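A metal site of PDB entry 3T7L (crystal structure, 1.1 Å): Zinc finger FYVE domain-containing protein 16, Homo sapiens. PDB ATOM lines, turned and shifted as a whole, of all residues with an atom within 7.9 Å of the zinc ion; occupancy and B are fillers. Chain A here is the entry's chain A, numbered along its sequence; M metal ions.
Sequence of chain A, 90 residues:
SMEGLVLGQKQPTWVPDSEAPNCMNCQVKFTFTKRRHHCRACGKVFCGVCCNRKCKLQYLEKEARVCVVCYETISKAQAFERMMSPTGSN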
ATOM      1  N   LEU A   7       4.178 -30.281  -6.577  1.00  0.00           N
ATOM      2  CA  LEU A   7       4.240 -28.969  -7.221  1.00  0.00           C
ATOM      3  C   LEU A   7       5.619 -28.370  -7.111  1.00  0.00           C
ATOM      4  O   LEU A   7       6.181 -28.270  -6.010  1.00  0.00           O
ATOM      5  CB  LEU A   7       3.204 -27.990  -6.654  1.00  0.00           C
ATOM      6  CG  LEU A   7       1.756 -28.279  -7.024  1.00  0.00           C
ATOM      7  CD1 LEU A   7       0.838 -27.213  -6.358  1.00  0.00           C
ATOM      8  CD2 LEU A   7       1.544 -28.251  -8.553  1.00  0.00           C
ATOM      9  N   PRO A  12       5.136 -29.540 -15.329  1.00  0.00           N
ATOM     10  CA  PRO A  12       3.797 -30.105 -15.601  1.00  0.00           C
ATOM     11  C   PRO A  12       3.523 -30.179 -17.103  1.00  0.00           C
ATOM     12  O   PRO A  12       4.178 -29.469 -17.868  1.00  0.00           O
ATOM     13  CB  PRO A  12       2.880 -29.069 -14.972  1.00  0.00           C
ATOM     14  CG  PRO A  12       3.636 -27.781 -15.164  1.00  0.00           C
ATOM     15  CD  PRO A  12       5.084 -28.132 -14.908  1.00  0.00           C
ATOM     16  N   HIS A  38      -0.052 -19.439 -18.554  1.00  0.00           N
ATOM     17  CA  HIS A  38       0.097 -20.735 -17.918  1.00  0.00           C
ATOM     18  C   HIS A  38       0.776 -20.643 -16.562  1.00  0.00           C
ATOM     19  O   HIS A  38       1.742 -19.880 -16.362  1.00  0.00           O
ATOM     20  CB  HIS A  38       0.936 -21.701 -18.776  1.00  0.00           C
ATOM     21  CG  HIS A  38       0.205 -22.238 -19.952  1.00  0.00           C
ATOM     22  ND1 HIS A  38       0.027 -21.528 -21.131  1.00  0.00           N
ATOM     23  CD2 HIS A  38      -0.389 -23.432 -20.137  1.00  0.00           C
ATOM     24  CE1 HIS A  38      -0.611 -22.301 -22.007  1.00  0.00           C
ATOM     25  NE2 HIS A  38      -0.908 -23.437 -21.410  1.00  0.00           N
ATOM     26  N   CYS A  39       0.305 -21.453 -15.643  1.00  0.00           N
ATOM     27  CA  CYS A  39       0.983 -21.683 -14.372  1.00  0.00           C
ATOM     28  C   CYS A  39       2.123 -22.650 -14.601  1.00  0.00           C
ATOM     29  O   CYS A  39       1.915 -23.761 -15.115  1.00  0.00           O
ATOM     30  CB  CYS A  39       0.002 -22.272 -13.353  1.00  0.00           C
ATOM     31  SG  CYS A  39       0.798 -22.689 -11.796  1.00  0.00           S
ATOM     32  N   ARG A  40       3.333 -22.283 -14.209  1.00  0.00           N
ATOM     33  CA  ARG A  40       4.488 -23.133 -14.388  1.00  0.00           C
ATOM     34  C   ARG A  40       4.534 -24.285 -13.400  1.00  0.00           C
ATOM     35  O   ARG A  40       5.356 -25.204 -13.539  1.00  0.00           O
ATOM     36  CB  ARG A  40       5.768 -22.293 -14.360  1.00  0.00           C
ATOM     37  CG  ARG A  40       6.161 -21.679 -15.657  1.00  0.00           C
ATOM     38  CD  ARG A  40       5.201 -20.683 -16.184  1.00  0.00           C
ATOM     39  NE  ARG A  40       5.792 -19.977 -17.305  1.00  0.00           N
ATOM     40  CZ  ARG A  40       5.151 -19.105 -18.063  1.00  0.00           C
ATOM     41  NH1 ARG A  40       3.900 -18.778 -17.872  1.00  0.00           N
ATOM     42  NH2 ARG A  40       5.806 -18.534 -19.085  1.00  0.00           N
ATOM     43  N   ALA A  41       3.687 -24.261 -12.373  1.00  0.00           N
ATOM     44  CA  ALA A  41       3.621 -25.375 -11.444  1.00  0.00           C
ATOM     45  C   ALA A  41       2.607 -26.450 -11.833  1.00  0.00           C
ATOM     46  O   ALA A  41       2.938 -27.638 -11.769  1.00  0.00           O
ATOM     47  CB  ALA A  41       3.373 -24.884 -10.002  1.00  0.00           C
ATOM     48  N   CYS A  42       1.412 -26.071 -12.270  1.00  0.00           N
ATOM     49  CA  CYS A  42       0.363 -27.027 -12.587  1.00  0.00           C
ATOM     50  C   CYS A  42       0.043 -27.151 -14.067  1.00  0.00           C
ATOM     51  O   CYS A  42      -0.639 -28.113 -14.449  1.00  0.00           O
ATOM     52  CB  CYS A  42      -0.930 -26.778 -11.792  1.00  0.00           C
ATOM     53  SG  CYS A  42      -1.814 -25.248 -12.282  1.00  0.00           S
ATOM     54  N   GLY A  43       0.518 -26.243 -14.887  1.00  0.00           N
ATOM     55  CA  GLY A  43       0.324 -26.328 -16.336  1.00  0.00           C
ATOM     56  C   GLY A  43      -1.021 -25.881 -16.860  1.00  0.00           C
ATOM     57  O   GLY A  43      -1.232 -25.883 -18.060  1.00  0.00           O
ATOM     58  N   LYS A  44      -1.929 -25.492 -15.970  1.00  0.00           N
ATOM     59  CA  LYS A  44      -3.243 -25.018 -16.356  1.00  0.00           C
ATOM     60  C   LYS A  44      -3.149 -23.569 -16.839  1.00  0.00           C
ATOM     61  O   LYS A  44      -2.102 -22.914 -16.766  1.00  0.00           O
ATOM     62  CB  LYS A  44      -4.232 -25.225 -15.216  1.00  0.00           C
ATOM     63  CG  LYS A  44      -4.575 -26.729 -15.035  1.00  0.00           C
ATOM     64  CD  LYS A  44      -5.794 -27.003 -14.245  1.00  0.00           C
ATOM     65  CE  LYS A  44      -5.728 -26.379 -12.873  1.00  0.00           C
ATOM     66  NZ  LYS A  44      -6.725 -26.855 -11.891  1.00  0.00           N
ATOM     67  N   VAL A  45      -4.250 -23.077 -17.387  1.00  0.00           N
ATOM     68  CA  VAL A  45      -4.309 -21.807 -18.113  1.00  0.00           C
ATOM     69  C   VAL A  45      -5.267 -20.862 -17.422  1.00  0.00           C
ATOM     70  O   VAL A  45      -6.382 -21.240 -17.076  1.00  0.00           O
ATOM     71  CB  VAL A  45      -4.764 -22.005 -19.557  1.00  0.00           C
ATOM     72  CG1 VAL A  45      -4.535 -20.743 -20.367  1.00  0.00           C
ATOM     73  CG2 VAL A  45      -4.027 -23.210 -20.220  1.00  0.00           C
ATOM     74  N   PHE A  46      -4.787 -19.643 -17.183  1.00  0.00           N
ATOM     75  CA  PHE A  46      -5.456 -18.664 -16.332  1.00  0.00           C
ATOM     76  C   PHE A  46      -5.461 -17.284 -16.926  1.00  0.00           C
ATOM     77  O   PHE A  46      -4.603 -16.953 -17.738  1.00  0.00           O
ATOM     78  CB  PHE A  46      -4.711 -18.612 -14.988  1.00  0.00           C
ATOM     79  CG  PHE A  46      -4.671 -19.918 -14.275  1.00  0.00           C
ATOM     80  CD1 PHE A  46      -3.614 -20.801 -14.472  1.00  0.00           C
ATOM     81  CD2 PHE A  46      -5.717 -20.320 -13.478  1.00  0.00           C
ATOM     82  CE1 PHE A  46      -3.596 -22.035 -13.835  1.00  0.00           C
ATOM     83  CE2 PHE A  46      -5.707 -21.553 -12.833  1.00  0.00           C
ATOM     84  CZ  PHE A  46      -4.629 -22.426 -13.041  1.00  0.00           C
ATOM     85  N   CYS A  50      -5.803 -14.291 -11.970  1.00  0.00           N
ATOM     86  CA  CYS A  50      -5.653 -15.593 -11.318  1.00  0.00           C
ATOM     87  C   CYS A  50      -4.267 -16.152 -11.408  1.00  0.00           C
ATOM     88  O   CYS A  50      -4.002 -17.193 -10.789  1.00  0.00           O
ATOM     89  CB  CYS A  50      -6.667 -16.579 -11.891  1.00  0.00           C
ATOM     90  SG  CYS A  50      -8.408 -16.102 -11.597  1.00  0.00           S
ATOM     91  N   CYS A  51      -3.363 -15.511 -12.117  1.00  0.00           N
ATOM     92  CA  CYS A  51      -2.019 -16.050 -12.321  1.00  0.00           C
ATOM     93  C   CYS A  51      -1.063 -14.936 -12.612  1.00  0.00           C
ATOM     94  O   CYS A  51      -0.782 -14.647 -13.765  1.00  0.00           O
ATOM     95  CB  CYS A  51      -2.059 -17.075 -13.445  1.00  0.00           C
ATOM     96  SG  CYS A  51      -0.547 -17.964 -13.818  1.00  0.00           S
ATOM     97  N   ARG A  65       6.011 -17.756 -13.046  1.00  0.00           N
ATOM     98  CA  ARG A  65       4.619 -17.426 -12.838  1.00  0.00           C
ATOM     99  C   ARG A  65       3.809 -18.626 -12.404  1.00  0.00           C
ATOM    100  O   ARG A  65       3.908 -19.726 -13.015  1.00  0.00           O
ATOM    101  CB  ARG A  65       4.015 -16.862 -14.124  1.00  0.00           C
ATOM    102  CG  ARG A  65       2.613 -16.357 -13.997  1.00  0.00           C
ATOM    103  CD  ARG A  65       1.991 -16.074 -15.364  1.00  0.00           C
ATOM    104  NE  ARG A  65       2.642 -14.968 -16.033  1.00  0.00           N
ATOM    105  CZ  ARG A  65       2.194 -13.720 -16.066  1.00  0.00           C
ATOM    106  NH1 ARG A  65       1.043 -13.389 -15.484  1.00  0.00           N
ATOM    107  NH2 ARG A  65       2.880 -12.792 -16.713  1.00  0.00           N
ATOM    108  N   VAL A  66       2.992 -18.439 -11.361  1.00  0.00           N
ATOM    109  CA  VAL A  66       2.132 -19.476 -10.837  1.00  0.00           C
ATOM    110  C   VAL A  66       0.721 -18.949 -10.540  1.00  0.00           C
ATOM    111  O   VAL A  66       0.534 -17.744 -10.342  1.00  0.00           O
ATOM    112  CB  VAL A  66       2.733 -20.110  -9.584  1.00  0.00           C
ATOM    113  CG1 VAL A  66       4.005 -20.892  -9.900  1.00  0.00           C
ATOM    114  CG2 VAL A  66       3.019 -19.073  -8.491  1.00  0.00           C
ATOM    115  N   CYS A  67      -0.248 -19.857 -10.535  1.00  0.00           N
ATOM    116  CA  CYS A  67      -1.628 -19.487 -10.295  1.00  0.00           C
ATOM    117  C   CYS A  67      -1.863 -19.257  -8.823  1.00  0.00           C
ATOM    118  O   CYS A  67      -1.038 -19.564  -7.944  1.00  0.00           O
ATOM    119  CB  CYS A  67      -2.566 -20.537 -10.853  1.00  0.00           C
ATOM    120  SG  CYS A  67      -2.604 -22.113  -9.915  1.00  0.00           S
ATOM    121  N   VAL A  68      -3.064 -18.768  -8.499  1.00  0.00           N
ATOM    122  CA  VAL A  68      -3.437 -18.452  -7.134  1.00  0.00           C
ATOM    123  C   VAL A  68      -3.324 -19.664  -6.198  1.00  0.00           C
ATOM    124  O   VAL A  68      -2.931 -19.566  -5.049  1.00  0.00           O
ATOM    125  CB  VAL A  68      -4.858 -17.838  -7.101  1.00  0.00           C
ATOM    126  CG1 VAL A  68      -5.878 -18.784  -7.757  1.00  0.00           C
ATOM    127  CG2 VAL A  68      -5.242 -17.422  -5.666  1.00  0.00           C
ATOM    128  N   VAL A  69      -3.713 -20.834  -6.722  1.00  0.00           N
ATOM    129  CA  VAL A  69      -3.690 -22.072  -5.938  1.00  0.00           C
ATOM    130  C   VAL A  69      -2.255 -22.510  -5.652  1.00  0.00           C
ATOM    131  O   VAL A  69      -1.858 -22.755  -4.509  1.00  0.00           O
ATOM    132  CB  VAL A  69      -4.467 -23.195  -6.678  1.00  0.00           C
ATOM    133  CG1 VAL A  69      -4.418 -24.511  -5.925  1.00  0.00           C
ATOM    134  CG2 VAL A  69      -5.871 -22.804  -6.997  1.00  0.00           C
ATOM    135  N   CYS A  70      -1.474 -22.611  -6.715  1.00  0.00           N
ATOM    136  CA  CYS A  70      -0.100 -23.066  -6.555  1.00  0.00           C
ATOM    137  C   CYS A  70       0.747 -22.083  -5.737  1.00  0.00           C
ATOM    138  O   CYS A  70       1.609 -22.488  -4.972  1.00  0.00           O
ATOM    139  CB  CYS A  70       0.533 -23.338  -7.914  1.00  0.00           C
ATOM    140  SG  CYS A  70      -0.217 -24.726  -8.806  1.00  0.00           S
ATOM    141  N   TYR A  71       0.503 -20.782  -5.875  1.00  0.00           N
ATOM    142  CA  TYR A  71       1.268 -19.789  -5.153  1.00  0.00           C
ATOM    143  C   TYR A  71       1.155 -20.036  -3.649  1.00  0.00           C
ATOM    144  O   TYR A  71       2.129 -20.060  -2.926  1.00  0.00           O
ATOM    145  CB  TYR A  71       0.808 -18.341  -5.456  1.00  0.00           C
ATOM    146  CG  TYR A  71       1.632 -17.349  -4.676  1.00  0.00           C
ATOM    147  CD1 TYR A  71       1.182 -16.839  -3.461  1.00  0.00           C
ATOM    148  CD2 TYR A  71       2.901 -16.990  -5.109  1.00  0.00           C
ATOM    149  CE1 TYR A  71       1.970 -15.964  -2.724  1.00  0.00           C
ATOM    150  CE2 TYR A  71       3.705 -16.133  -4.367  1.00  0.00           C
ATOM    151  CZ  TYR A  71       3.240 -15.632  -3.179  1.00  0.00           C
ATOM    152  OH  TYR A  71       4.049 -14.770  -2.460  1.00  0.00           O
ATOM    153  N   ILE A  74       2.766 -23.522  -2.621  1.00  0.00           N
ATOM    154  CA  ILE A  74       4.239 -23.534  -2.707  1.00  0.00           C
ATOM    155  C   ILE A  74       4.906 -22.533  -1.759  1.00  0.00           C
ATOM    156  O   ILE A  74       5.928 -22.864  -1.119  1.00  0.00           O
ATOM    157  CB  ILE A  74       4.723 -23.267  -4.137  1.00  0.00           C
ATOM    158  CG1 ILE A  74       4.224 -24.392  -5.013  1.00  0.00           C
ATOM    159  CG2 ILE A  74       6.267 -23.161  -4.189  1.00  0.00           C
ATOM    160  CD1 ILE A  74       4.354 -24.155  -6.486  1.00  0.00           C
HETATM  161 ZN    ZN M   1      -1.057 -23.697 -10.710  1.00  0.00          ZN
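The zinc ion is bound by SG of Cys 70 (2.3 Å). The side-chain sulfur (SG) of Cys 42 is bound to the zinc ion. The zinc ion is bound by SG of Cys 67 (2.4 Å). The zinc ion is bound by SG of Cys 39, at 2.4 Å. The zinc ion has four donor atoms within binding distance.
Four residues have an atom within 4 Å of the zinc ion: Cys 39, Cys 42, Cys 67 and Cys 70.
The side-chain sulfur (SG) of Cys 42 lies close to the backbone NH (N) of Lys 44. SG of Cys 67 sits close to N of Val 69. The backbone NH of Ala 41 sits close to the side-chain sulfur of Cys 39 (3.3 Å). The backbone NH (N) of Cys 39 lies within hydrogen-bond range of the backbone carbonyl oxygen (O) of Lys 44 (3.0 Å).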
